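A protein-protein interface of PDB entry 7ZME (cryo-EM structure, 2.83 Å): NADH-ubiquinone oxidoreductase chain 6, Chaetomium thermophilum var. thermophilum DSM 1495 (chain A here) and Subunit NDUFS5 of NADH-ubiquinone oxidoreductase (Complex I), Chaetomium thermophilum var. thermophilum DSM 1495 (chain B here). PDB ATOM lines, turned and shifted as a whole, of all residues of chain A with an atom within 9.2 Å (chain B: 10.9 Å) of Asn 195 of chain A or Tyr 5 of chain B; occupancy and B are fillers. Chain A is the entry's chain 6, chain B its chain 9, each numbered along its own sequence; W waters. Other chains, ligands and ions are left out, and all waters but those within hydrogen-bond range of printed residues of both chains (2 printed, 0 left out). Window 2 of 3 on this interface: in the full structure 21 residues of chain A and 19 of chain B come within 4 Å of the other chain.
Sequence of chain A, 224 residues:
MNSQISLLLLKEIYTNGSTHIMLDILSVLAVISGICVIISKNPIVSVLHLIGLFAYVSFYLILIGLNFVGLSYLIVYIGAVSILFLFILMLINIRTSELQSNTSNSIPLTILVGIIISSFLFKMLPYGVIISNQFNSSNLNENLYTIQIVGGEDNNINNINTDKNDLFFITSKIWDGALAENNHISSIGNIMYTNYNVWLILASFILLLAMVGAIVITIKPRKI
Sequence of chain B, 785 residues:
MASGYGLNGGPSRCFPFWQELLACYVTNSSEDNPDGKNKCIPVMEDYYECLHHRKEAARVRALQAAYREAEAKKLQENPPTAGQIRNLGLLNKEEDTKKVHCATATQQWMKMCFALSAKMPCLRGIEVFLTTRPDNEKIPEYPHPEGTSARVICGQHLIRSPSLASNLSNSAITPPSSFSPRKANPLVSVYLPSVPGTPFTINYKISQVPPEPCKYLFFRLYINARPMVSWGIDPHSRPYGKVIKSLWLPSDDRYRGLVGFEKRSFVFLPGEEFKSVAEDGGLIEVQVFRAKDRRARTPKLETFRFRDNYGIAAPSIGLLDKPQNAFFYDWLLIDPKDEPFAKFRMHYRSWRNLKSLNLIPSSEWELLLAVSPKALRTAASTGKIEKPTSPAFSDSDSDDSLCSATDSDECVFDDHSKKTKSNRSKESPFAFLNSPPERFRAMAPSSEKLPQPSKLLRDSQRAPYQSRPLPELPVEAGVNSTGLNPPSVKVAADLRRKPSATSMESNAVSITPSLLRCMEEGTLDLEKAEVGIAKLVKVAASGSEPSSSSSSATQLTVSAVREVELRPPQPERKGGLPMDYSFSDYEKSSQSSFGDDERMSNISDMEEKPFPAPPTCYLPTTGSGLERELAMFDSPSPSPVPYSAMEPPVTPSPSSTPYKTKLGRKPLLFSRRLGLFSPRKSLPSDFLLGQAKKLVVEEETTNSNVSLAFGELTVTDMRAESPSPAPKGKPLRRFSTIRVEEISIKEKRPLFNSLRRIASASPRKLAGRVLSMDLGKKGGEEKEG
Leu 7 of chain B touches His 184 of chain A.
Ser 187 of chain A touches Asn 8 of chain B (OG to C, 3.5 Å).
Tyr 5 of chain B touches Ile 191 of chain A (CD2 to CG2, 3.7 Å).
Tyr 196 of chain A touches Tyr 5 of chain B.
Of the printed residues of chain B, His 184 of chain A touches Leu 7 (3.3 Å).
No residue of chain B comes within 4 Å of Thr 194 of chain A.
Asn 195 of chain A touches one residue of chain B.
No residue of chain A comes within 4 Å of Ser 3 of chain B.
No residue of chain A comes within 4 Å of Gly 4 of chain B.
Of chain A, only Ile 191, Asn 195 and Tyr 196 come within 4 Å of Tyr 5 of chain B.
Printed residues of chain A within 4 Å of Gly 9 of chain B: Ser 187.
The nearest residue of chain B that does not touch Asn 195 of chain A is Ser 3 of chain B (7.4 Å).
The nearest residue of chain A that does not touch Tyr 5 of chain B is Ser 187 of chain A (5.9 Å).
Printed residues of chain B that touch a printed residue of chain A: Tyr 5, Leu 7, Asn 8 and Gly 9.
Hydrophobic or aromatic side chains of chain B that line the printed part of chain A: Tyr 5 and Leu 7.
Of the 15 printed residues of chain A, 5 touch a printed residue of chain B.
Hydrophobic or aromatic side chains of chain A that line the printed part of chain B: His 184, Ile 191 and Tyr 196.
The backbone carbonyl oxygen (O) of Ile 191 of chain A lies within hydrogen-bond range of the backbone NH (N) of Tyr 196 of chain A, 3.0 Å away.
OD1 of Asn 195 of chain A is in hydrogen-bond range of OG1 of Thr 194 of chain A, at 2.8 Å.
OD1 of Asn 8 of chain B sits at hydrogen-bond distance from N of Gly 10 of chain B, at 3.1 Å.
The side-chain hydroxyl (OG) of Ser 187 of chain A lies within hydrogen-bond range of the backbone NH (N) of Gly 9 of chain B (3.1 Å).
The side-chain hydroxyl (OG) of Ser 187 of chain A is in hydrogen-bond range of the backbone carbonyl oxygen (O) of Leu 7 of chain B (2.9 Å).
The side-chain amide nitrogen (ND2) of Asn 195 of chain A sits at hydrogen-bond distance from the side-chain hydroxyl (OH) of Tyr 5 of chain B (2.9 Å).
Water W2 lies within hydrogen-bond range of the side-chain hydroxyl (OH) of Tyr 5 of chain B (2.6 Å) and the side-chain amide nitrogen (ND2) of Asn 195 of chain A (3.0 Å).
Water W1 lies within hydrogen-bond range of the side-chain amide nitrogen of Asn 195 of chain A and the side-chain hydroxyl of Tyr 5 of chain B.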
ATOM      1  N   HIS A 184      11.965 -21.974 -12.418  1.00  0.00           N
ATOM      2  CA  HIS A 184      11.322 -21.798 -11.095  1.00  0.00           C
ATOM      3  C   HIS A 184      11.236 -20.314 -10.732  1.00  0.00           C
ATOM      4  O   HIS A 184      10.225 -19.920 -10.152  1.00  0.00           O
ATOM      5  CB  HIS A 184      12.085 -22.601 -10.042  1.00  0.00           C
ATOM      6  CG  HIS A 184      11.912 -24.078 -10.133  1.00  0.00           C
ATOM      7  ND1 HIS A 184      12.438 -24.936  -9.191  1.00  0.00           N
ATOM      8  CD2 HIS A 184      11.281 -24.852 -11.037  1.00  0.00           C
ATOM      9  CE1 HIS A 184      12.140 -26.174  -9.512  1.00  0.00           C
ATOM     10  NE2 HIS A 184      11.431 -26.150 -10.640  1.00  0.00           N
ATOM     11  N   SER A 187       8.334 -18.846 -12.439  1.00  0.00           N
ATOM     12  CA  SER A 187       7.078 -19.315 -11.807  1.00  0.00           C
ATOM     13  C   SER A 187       6.785 -18.500 -10.549  1.00  0.00           C
ATOM     14  O   SER A 187       5.604 -18.212 -10.301  1.00  0.00           O
ATOM     15  CB  SER A 187       7.145 -20.778 -11.518  1.00  0.00           C
ATOM     16  OG  SER A 187       7.602 -21.490 -12.654  1.00  0.00           O
ATOM     17  N   ILE A 188       7.824 -18.137  -9.799  1.00  0.00           N
ATOM     18  CA  ILE A 188       7.652 -17.319  -8.576  1.00  0.00           C
ATOM     19  C   ILE A 188       7.333 -15.901  -9.048  1.00  0.00           C
ATOM     20  O   ILE A 188       6.403 -15.312  -8.495  1.00  0.00           O
ATOM     21  CB  ILE A 188       8.949 -17.349  -7.752  1.00  0.00           C
ATOM     22  CG1 ILE A 188       9.221 -18.729  -7.150  1.00  0.00           C
ATOM     23  CG2 ILE A 188       8.955 -16.264  -6.686  1.00  0.00           C
ATOM     24  CD1 ILE A 188      10.629 -18.918  -6.654  1.00  0.00           C
ATOM     25  N   GLY A 189       7.995 -15.420 -10.100  1.00  0.00           N
ATOM     26  CA  GLY A 189       7.672 -14.096 -10.598  1.00  0.00           C
ATOM     27  C   GLY A 189       6.256 -13.973 -11.118  1.00  0.00           C
ATOM     28  O   GLY A 189       5.661 -12.895 -11.054  1.00  0.00           O
ATOM     29  N   ASN A 190       5.697 -15.067 -11.640  1.00  0.00           N
ATOM     30  CA  ASN A 190       4.329 -15.047 -12.145  1.00  0.00           C
ATOM     31  C   ASN A 190       3.317 -14.669 -11.072  1.00  0.00           C
ATOM     32  O   ASN A 190       2.240 -14.163 -11.402  1.00  0.00           O
ATOM     33  CB  ASN A 190       3.966 -16.412 -12.729  1.00  0.00           C
ATOM     34  CG  ASN A 190       4.615 -16.670 -14.077  1.00  0.00           C
ATOM     35  OD1 ASN A 190       4.597 -17.792 -14.578  1.00  0.00           O
ATOM     36  ND2 ASN A 190       5.190 -15.635 -14.669  1.00  0.00           N
ATOM     37  N   ILE A 191       3.638 -14.899  -9.801  1.00  0.00           N
ATOM     38  CA  ILE A 191       2.691 -14.690  -8.709  1.00  0.00           C
ATOM     39  C   ILE A 191       3.216 -13.773  -7.620  1.00  0.00           C
ATOM     40  O   ILE A 191       2.421 -13.264  -6.811  1.00  0.00           O
ATOM     41  CB  ILE A 191       2.286 -16.047  -8.103  1.00  0.00           C
ATOM     42  CG1 ILE A 191       3.534 -16.753  -7.582  1.00  0.00           C
ATOM     43  CG2 ILE A 191       1.579 -16.902  -9.129  1.00  0.00           C
ATOM     44  CD1 ILE A 191       3.249 -17.932  -6.737  1.00  0.00           C
ATOM     45  N   MET A 192       4.522 -13.530  -7.545  1.00  0.00           N
ATOM     46  CA  MET A 192       5.110 -12.780  -6.444  1.00  0.00           C
ATOM     47  C   MET A 192       4.721 -11.307  -6.465  1.00  0.00           C
ATOM     48  O   MET A 192       4.827 -10.630  -5.436  1.00  0.00           O
ATOM     49  CB  MET A 192       6.628 -12.961  -6.500  1.00  0.00           C
ATOM     50  CG  MET A 192       7.467 -12.020  -5.679  1.00  0.00           C
ATOM     51  SD  MET A 192       9.191 -12.248  -6.108  1.00  0.00           S
ATOM     52  CE  MET A 192       9.978 -11.538  -4.681  1.00  0.00           C
ATOM     53  N   TYR A 193       4.259 -10.800  -7.603  1.00  0.00           N
ATOM     54  CA  TYR A 193       3.997  -9.343  -7.707  1.00  0.00           C
ATOM     55  C   TYR A 193       2.523  -9.096  -8.017  1.00  0.00           C
ATOM     56  O   TYR A 193       2.150  -7.949  -8.273  1.00  0.00           O
ATOM     57  CB  TYR A 193       4.908  -8.722  -8.767  1.00  0.00           C
ATOM     58  CG  TYR A 193       6.374  -9.038  -8.619  1.00  0.00           C
ATOM     59  CD1 TYR A 193       7.197  -8.250  -7.838  1.00  0.00           C
ATOM     60  CD2 TYR A 193       6.933 -10.126  -9.263  1.00  0.00           C
ATOM     61  CE1 TYR A 193       8.543  -8.535  -7.695  1.00  0.00           C
ATOM     62  CE2 TYR A 193       8.273 -10.432  -9.125  1.00  0.00           C
ATOM     63  CZ  TYR A 193       9.082  -9.629  -8.343  1.00  0.00           C
ATOM     64  OH  TYR A 193      10.405  -9.924  -8.217  1.00  0.00           O
ATOM     65  N   THR A 194       1.714 -10.150  -8.009  1.00  0.00           N
ATOM     66  CA  THR A 194       0.259  -9.990  -8.218  1.00  0.00           C
ATOM     67  C   THR A 194      -0.491 -10.795  -7.172  1.00  0.00           C
ATOM     68  O   THR A 194      -0.961 -10.179  -6.223  1.00  0.00           O
ATOM     69  CB  THR A 194      -0.161 -10.461  -9.615  1.00  0.00           C
ATOM     70  OG1 THR A 194       0.306 -11.789  -9.845  1.00  0.00           O
ATOM     71  CG2 THR A 194       0.336  -9.552 -10.718  1.00  0.00           C
ATOM     72  N   ASN A 195      -0.500 -12.118  -7.286  1.00  0.00           N
ATOM     73  CA  ASN A 195      -1.316 -13.000  -6.410  1.00  0.00           C
ATOM     74  C   ASN A 195      -0.903 -12.856  -4.946  1.00  0.00           C
ATOM     75  O   ASN A 195      -1.784 -12.924  -4.084  1.00  0.00           O
ATOM     76  CB  ASN A 195      -1.200 -14.446  -6.885  1.00  0.00           C
ATOM     77  CG  ASN A 195      -1.584 -14.662  -8.333  1.00  0.00           C
ATOM     78  OD1 ASN A 195      -0.878 -14.243  -9.243  1.00  0.00           O
ATOM     79  ND2 ASN A 195      -2.692 -15.345  -8.557  1.00  0.00           N
ATOM     80  N   TYR A 196       0.389 -12.685  -4.680  1.00  0.00           N
ATOM     81  CA  TYR A 196       0.901 -12.614  -3.290  1.00  0.00           C
ATOM     82  C   TYR A 196       1.623 -11.282  -3.045  1.00  0.00           C
ATOM     83  O   TYR A 196       2.556 -11.272  -2.243  1.00  0.00           O
ATOM     84  CB  TYR A 196       1.704 -13.882  -2.987  1.00  0.00           C
ATOM     85  CG  TYR A 196       0.911 -15.148  -3.189  1.00  0.00           C
ATOM     86  CD1 TYR A 196       0.107 -15.654  -2.183  1.00  0.00           C
ATOM     87  CD2 TYR A 196       0.921 -15.814  -4.402  1.00  0.00           C
ATOM     88  CE1 TYR A 196      -0.642 -16.803  -2.365  1.00  0.00           C
ATOM     89  CE2 TYR A 196       0.161 -16.951  -4.609  1.00  0.00           C
ATOM     90  CZ  TYR A 196      -0.619 -17.454  -3.584  1.00  0.00           C
ATOM     91  OH  TYR A 196      -1.357 -18.585  -3.776  1.00  0.00           O
ATOM     92  N   ASN A 197       1.179 -10.191  -3.669  1.00  0.00           N
ATOM     93  CA  ASN A 197       1.859  -8.869  -3.560  1.00  0.00           C
ATOM     94  C   ASN A 197       1.874  -8.342  -2.115  1.00  0.00           C
ATOM     95  O   ASN A 197       2.723  -7.499  -1.826  1.00  0.00           O
ATOM     96  CB  ASN A 197       1.332  -7.865  -4.596  1.00  0.00           C
ATOM     97  CG  ASN A 197      -0.117  -7.453  -4.432  1.00  0.00           C
ATOM     98  OD1 ASN A 197      -0.658  -7.452  -3.331  1.00  0.00           O
ATOM     99  ND2 ASN A 197      -0.744  -7.065  -5.528  1.00  0.00           N
ATOM    100  N   VAL A 198       0.940  -8.843  -1.261  1.00  0.00           N
ATOM    101  CA  VAL A 198       0.843  -8.389   0.151  1.00  0.00           C
ATOM    102  C   VAL A 198       2.097  -8.849   0.877  1.00  0.00           C
ATOM    103  O   VAL A 198       2.654  -8.054   1.630  1.00  0.00           O
ATOM    104  CB  VAL A 198      -0.455  -8.871   0.838  1.00  0.00           C
ATOM    105  CG1 VAL A 198      -0.250  -9.274   2.291  1.00  0.00           C
ATOM    106  CG2 VAL A 198      -1.573  -7.850   0.715  1.00  0.00           C
ATOM    107  N   TRP A 199       2.563 -10.035   0.611  1.00  0.00           N
ATOM    108  CA  TRP A 199       3.798 -10.491   1.232  1.00  0.00           C
ATOM    109  C   TRP A 199       4.975  -9.615   0.838  1.00  0.00           C
ATOM    110  O   TRP A 199       5.915  -9.455   1.620  1.00  0.00           O
ATOM    111  CB  TRP A 199       4.071 -11.940   0.849  1.00  0.00           C
ATOM    112  CG  TRP A 199       3.053 -12.892   1.359  1.00  0.00           C
ATOM    113  CD1 TRP A 199       2.131 -12.663   2.333  1.00  0.00           C
ATOM    114  CD2 TRP A 199       2.852 -14.235   0.921  1.00  0.00           C
ATOM    115  NE1 TRP A 199       1.365 -13.781   2.531  1.00  0.00           N
ATOM    116  CE2 TRP A 199       1.788 -14.763   1.676  1.00  0.00           C
ATOM    117  CE3 TRP A 199       3.469 -15.045  -0.035  1.00  0.00           C
ATOM    118  CZ2 TRP A 199       1.324 -16.059   1.502  1.00  0.00           C
ATOM    119  CZ3 TRP A 199       3.008 -16.330  -0.205  1.00  0.00           C
ATOM    120  CH2 TRP A 199       1.947 -16.828   0.561  1.00  0.00           C
ATOM    121  N   LEU A 200       4.943  -9.045  -0.367  1.00  0.00           N
ATOM    122  CA  LEU A 200       6.018  -8.165  -0.804  1.00  0.00           C
ATOM    123  C   LEU A 200       5.954  -6.815  -0.098  1.00  0.00           C
ATOM    124  O   LEU A 200       6.990  -6.258   0.279  1.00  0.00           O
ATOM    125  CB  LEU A 200       5.958  -7.993  -2.318  1.00  0.00           C
ATOM    126  CG  LEU A 200       7.090  -7.240  -3.016  1.00  0.00           C
ATOM    127  CD1 LEU A 200       8.372  -8.057  -3.039  1.00  0.00           C
ATOM    128  CD2 LEU A 200       6.663  -6.873  -4.425  1.00  0.00           C
ATOM    129  N   MET B   1       0.386 -28.620  -4.400  1.00  0.00           N
ATOM    130  CA  MET B   1      -0.627 -28.785  -3.367  1.00  0.00           C
ATOM    131  C   MET B   1      -1.767 -27.791  -3.523  1.00  0.00           C
ATOM    132  O   MET B   1      -2.264 -27.571  -4.625  1.00  0.00           O
ATOM    133  CB  MET B   1      -0.005 -28.643  -1.981  1.00  0.00           C
ATOM    134  N   ALA B   2      -2.167 -27.186  -2.408  1.00  0.00           N
ATOM    135  CA  ALA B   2      -3.422 -26.446  -2.325  1.00  0.00           C
ATOM    136  C   ALA B   2      -3.368 -25.071  -2.970  1.00  0.00           C
ATOM    137  O   ALA B   2      -4.418 -24.436  -3.086  1.00  0.00           O
ATOM    138  CB  ALA B   2      -3.841 -26.306  -0.863  1.00  0.00           C
ATOM    139  N   SER B   3      -2.200 -24.586  -3.379  1.00  0.00           N
ATOM    140  CA  SER B   3      -2.106 -23.241  -3.930  1.00  0.00           C
ATOM    141  C   SER B   3      -2.646 -23.137  -5.353  1.00  0.00           C
ATOM    142  O   SER B   3      -3.353 -22.179  -5.674  1.00  0.00           O
ATOM    143  CB  SER B   3      -0.655 -22.757  -3.888  1.00  0.00           C
ATOM    144  OG  SER B   3       0.230 -23.658  -4.536  1.00  0.00           O
ATOM    145  N   GLY B   4      -2.338 -24.102  -6.210  1.00  0.00           N
ATOM    146  CA  GLY B   4      -2.708 -24.028  -7.603  1.00  0.00           C
ATOM    147  C   GLY B   4      -1.633 -23.513  -8.527  1.00  0.00           C
ATOM    148  O   GLY B   4      -1.918 -23.276  -9.704  1.00  0.00           O
ATOM    149  N   TYR B   5      -0.448 -23.272  -7.975  1.00  0.00           N
ATOM    150  CA  TYR B   5       0.685 -22.711  -8.743  1.00  0.00           C
ATOM    151  C   TYR B   5       1.863 -23.650  -8.520  1.00  0.00           C
ATOM    152  O   TYR B   5       2.402 -23.677  -7.426  1.00  0.00           O
ATOM    153  CB  TYR B   5       0.932 -21.272  -8.293  1.00  0.00           C
ATOM    154  CG  TYR B   5      -0.287 -20.396  -8.394  1.00  0.00           C
ATOM    155  CD1 TYR B   5      -1.131 -20.221  -7.309  1.00  0.00           C
ATOM    156  CD2 TYR B   5      -0.627 -19.779  -9.584  1.00  0.00           C
ATOM    157  CE1 TYR B   5      -2.274 -19.449  -7.400  1.00  0.00           C
ATOM    158  CE2 TYR B   5      -1.760 -18.994  -9.688  1.00  0.00           C
ATOM    159  CZ  TYR B   5      -2.587 -18.832  -8.594  1.00  0.00           C
ATOM    160  OH  TYR B   5      -3.711 -18.062  -8.677  1.00  0.00           O
ATOM    161  N   GLY B   6       2.193 -24.450  -9.518  1.00  0.00           N
ATOM    162  CA  GLY B   6       3.278 -25.433  -9.425  1.00  0.00           C
ATOM    163  C   GLY B   6       4.632 -24.930  -9.872  1.00  0.00           C
ATOM    164  O   GLY B   6       4.743 -23.754 -10.235  1.00  0.00           O
ATOM    165  N   LEU B   7       5.612 -25.823  -9.940  1.00  0.00           N
ATOM    166  CA  LEU B   7       7.022 -25.464 -10.247  1.00  0.00           C
ATOM    167  C   LEU B   7       7.273 -24.966 -11.678  1.00  0.00           C
ATOM    168  O   LEU B   7       8.202 -24.157 -11.843  1.00  0.00           O
ATOM    169  CB  LEU B   7       7.917 -26.632  -9.831  1.00  0.00           C
ATOM    170  CG  LEU B   7       7.738 -27.081  -8.383  1.00  0.00           C
ATOM    171  CD1 LEU B   7       8.549 -28.330  -8.089  1.00  0.00           C
ATOM    172  CD2 LEU B   7       8.103 -25.968  -7.420  1.00  0.00           C
ATOM    173  N   ASN B   8       6.511 -25.430 -12.673  1.00  0.00           N
ATOM    174  CA  ASN B   8       6.814 -25.095 -14.095  1.00  0.00           C
ATOM    175  C   ASN B   8       6.008 -23.921 -14.652  1.00  0.00           C
ATOM    176  O   ASN B   8       6.108 -23.685 -15.857  1.00  0.00           O
ATOM    177  CB  ASN B   8       6.751 -26.318 -15.010  1.00  0.00           C
ATOM    178  CG  ASN B   8       5.370 -26.908 -15.211  1.00  0.00           C
ATOM    179  OD1 ASN B   8       4.502 -26.298 -15.829  1.00  0.00           O
ATOM    180  ND2 ASN B   8       5.170 -28.127 -14.738  1.00  0.00           N
ATOM    181  N   GLY B   9       5.246 -23.217 -13.827  1.00  0.00           N
ATOM    182  CA  GLY B   9       4.374 -22.140 -14.328  1.00  0.00           C
ATOM    183  C   GLY B   9       3.008 -22.696 -14.602  1.00  0.00           C
ATOM    184  O   GLY B   9       2.126 -21.911 -14.918  1.00  0.00           O
ATOM    185  N   GLY B  10       2.868 -24.018 -14.527  1.00  0.00           N
ATOM    186  CA  GLY B  10       1.557 -24.662 -14.635  1.00  0.00           C
ATOM    187  C   GLY B  10       0.986 -24.861 -13.248  1.00  0.00           C
ATOM    188  O   GLY B  10       1.610 -24.426 -12.286  1.00  0.00           O
ATOM    189  N   PRO B  11      -0.190 -25.497 -13.108  1.00  0.00           N
ATOM    190  CA  PRO B  11      -0.845 -25.659 -11.812  1.00  0.00           C
ATOM    191  C   PRO B  11      -0.310 -26.821 -10.968  1.00  0.00           C
ATOM    192  O   PRO B  11       0.350 -27.667 -11.507  1.00  0.00           O
ATOM    193  CB  PRO B  11      -2.292 -25.969 -12.211  1.00  0.00           C
ATOM    194  CG  PRO B  11      -2.374 -25.783 -13.706  1.00  0.00           C
ATOM    195  CD  PRO B  11      -0.976 -26.047 -14.204  1.00  0.00           C
ATOM    196  N   SER B  12      -0.540 -26.795  -9.664  1.00  0.00           N
ATOM    197  CA  SER B  12       0.012 -27.790  -8.709  1.00  0.00           C
ATOM    198  C   SER B  12      -0.682 -29.146  -8.914  1.00  0.00           C
ATOM    199  O   SER B  12      -1.859 -29.145  -9.261  1.00  0.00           O
ATOM    200  CB  SER B  12      -0.042 -27.271  -7.290  1.00  0.00           C
ATOM    201  OG  SER B  12      -1.342 -26.835  -6.946  1.00  0.00           O
ATOM    202  N   ARG B  13       0.008 -30.254  -8.674  1.00  0.00           N
ATOM    203  CA  ARG B  13      -0.563 -31.615  -8.894  1.00  0.00           C
ATOM    204  C   ARG B  13      -1.746 -31.895  -7.963  1.00  0.00           C
ATOM    205  O   ARG B  13      -2.662 -32.593  -8.396  1.00  0.00           O
ATOM    206  CB  ARG B  13       0.511 -32.706  -8.847  1.00  0.00           C
ATOM    207  CG  ARG B  13       1.420 -32.644  -7.634  1.00  0.00           C
ATOM    208  CD  ARG B  13       2.419 -33.780  -7.650  1.00  0.00           C
ATOM    209  NE  ARG B  13       2.898 -33.961  -6.295  1.00  0.00           N
ATOM    210  CZ  ARG B  13       2.320 -34.771  -5.427  1.00  0.00           C
ATOM    211  NH1 ARG B  13       2.794 -34.879  -4.200  1.00  0.00           N
ATOM    212  NH2 ARG B  13       1.268 -35.476  -5.798  1.00  0.00           N
ATOM    213  N   CYS B  14      -1.706 -31.431  -6.720  1.00  0.00           N
ATOM    214  CA  CYS B  14      -2.790 -31.769  -5.763  1.00  0.00           C
ATOM    215  C   CYS B  14      -3.819 -30.643  -5.710  1.00  0.00           C
ATOM    216  O   CYS B  14      -4.520 -30.566  -4.711  1.00  0.00           O
ATOM    217  CB  CYS B  14      -2.207 -32.055  -4.383  1.00  0.00           C
ATOM    218  SG  CYS B  14      -1.194 -33.547  -4.364  1.00  0.00           S
ATOM    219  N   PHE B  15      -3.888 -29.812  -6.743  1.00  0.00           N
ATOM    220  CA  PHE B  15      -4.901 -28.769  -6.742  1.00  0.00           C
ATOM    221  C   PHE B  15      -6.296 -29.287  -7.084  1.00  0.00           C
ATOM    222  O   PHE B  15      -7.267 -28.842  -6.461  1.00  0.00           O
ATOM    223  CB  PHE B  15      -4.511 -27.645  -7.699  1.00  0.00           C
ATOM    224  CG  PHE B  15      -5.316 -26.400  -7.511  1.00  0.00           C
ATOM    225  CD1 PHE B  15      -5.409 -25.809  -6.265  1.00  0.00           C
ATOM    226  CD2 PHE B  15      -5.994 -25.831  -8.570  1.00  0.00           C
ATOM    227  CE1 PHE B  15      -6.156 -24.672  -6.085  1.00  0.00           C
ATOM    228  CE2 PHE B  15      -6.739 -24.693  -8.391  1.00  0.00           C
ATOM    229  CZ  PHE B  15      -6.817 -24.111  -7.150  1.00  0.00           C
ATOM    230  N   PRO B  16      -6.487 -30.221  -8.056  1.00  0.00           N
ATOM    231  CA  PRO B  16      -7.811 -30.798  -8.293  1.00  0.00           C
ATOM    232  C   PRO B  16      -8.359 -31.490  -7.038  1.00  0.00           C
ATOM    233  O   PRO B  16      -9.515 -31.349  -6.776  1.00  0.00           O
ATOM    234  CB  PRO B  16      -7.533 -31.859  -9.357  1.00  0.00           C
ATOM    235  CG  PRO B  16      -6.379 -31.328 -10.126  1.00  0.00           C
ATOM    236  CD  PRO B  16      -5.514 -30.758  -9.036  1.00  0.00           C
ATOM    237  N   TRP B  18      -7.741 -30.725  -3.975  1.00  0.00           N
ATOM    238  CA  TRP B  18      -8.066 -29.686  -2.964  1.00  0.00           C
ATOM    239  C   TRP B  18      -9.357 -28.968  -3.355  1.00  0.00           C
ATOM    240  O   TRP B  18     -10.180 -28.711  -2.473  1.00  0.00           O
ATOM    241  CB  TRP B  18      -6.892 -28.711  -2.877  1.00  0.00           C
ATOM    242  CG  TRP B  18      -7.120 -27.529  -1.988  1.00  0.00           C
ATOM    243  CD1 TRP B  18      -7.304 -26.234  -2.374  1.00  0.00           C
ATOM    244  CD2 TRP B  18      -7.177 -27.533  -0.552  1.00  0.00           C
ATOM    245  NE1 TRP B  18      -7.469 -25.433  -1.279  1.00  0.00           N
ATOM    246  CE2 TRP B  18      -7.401 -26.201  -0.147  1.00  0.00           C
ATOM    247  CE3 TRP B  18      -7.064 -28.525   0.426  1.00  0.00           C
ATOM    248  CZ2 TRP B  18      -7.508 -25.841   1.193  1.00  0.00           C
ATOM    249  CZ3 TRP B  18      -7.167 -28.168   1.751  1.00  0.00           C
ATOM    250  CH2 TRP B  18      -7.389 -26.845   2.127  1.00  0.00           C
ATOM    251  N   GLN B  19      -9.525 -28.662  -4.636  1.00  0.00           N
ATOM    252  CA  GLN B  19     -10.718 -27.930  -5.125  1.00  0.00           C
ATOM    253  C   GLN B  19     -11.938 -28.823  -4.938  1.00  0.00           C
ATOM    254  O   GLN B  19     -12.995 -28.292  -4.600  1.00  0.00           O
ATOM    255  CB  GLN B  19     -10.502 -27.434  -6.555  1.00  0.00           C
ATOM    256  CG  GLN B  19      -9.500 -26.302  -6.655  1.00  0.00           C
ATOM    257  CD  GLN B  19     -10.153 -24.943  -6.671  1.00  0.00           C
ATOM    258  OE1 GLN B  19     -10.752 -24.538  -7.661  1.00  0.00           O
ATOM    259  NE2 GLN B  19     -10.015 -24.211  -5.577  1.00  0.00           N
HETATM  260  O   HOH W   1      -3.689 -16.122  -5.948  1.00  0.00           O
HETATM  261  O   HOH W   2      -3.719 -16.885 -10.968  1.00  0.00           O
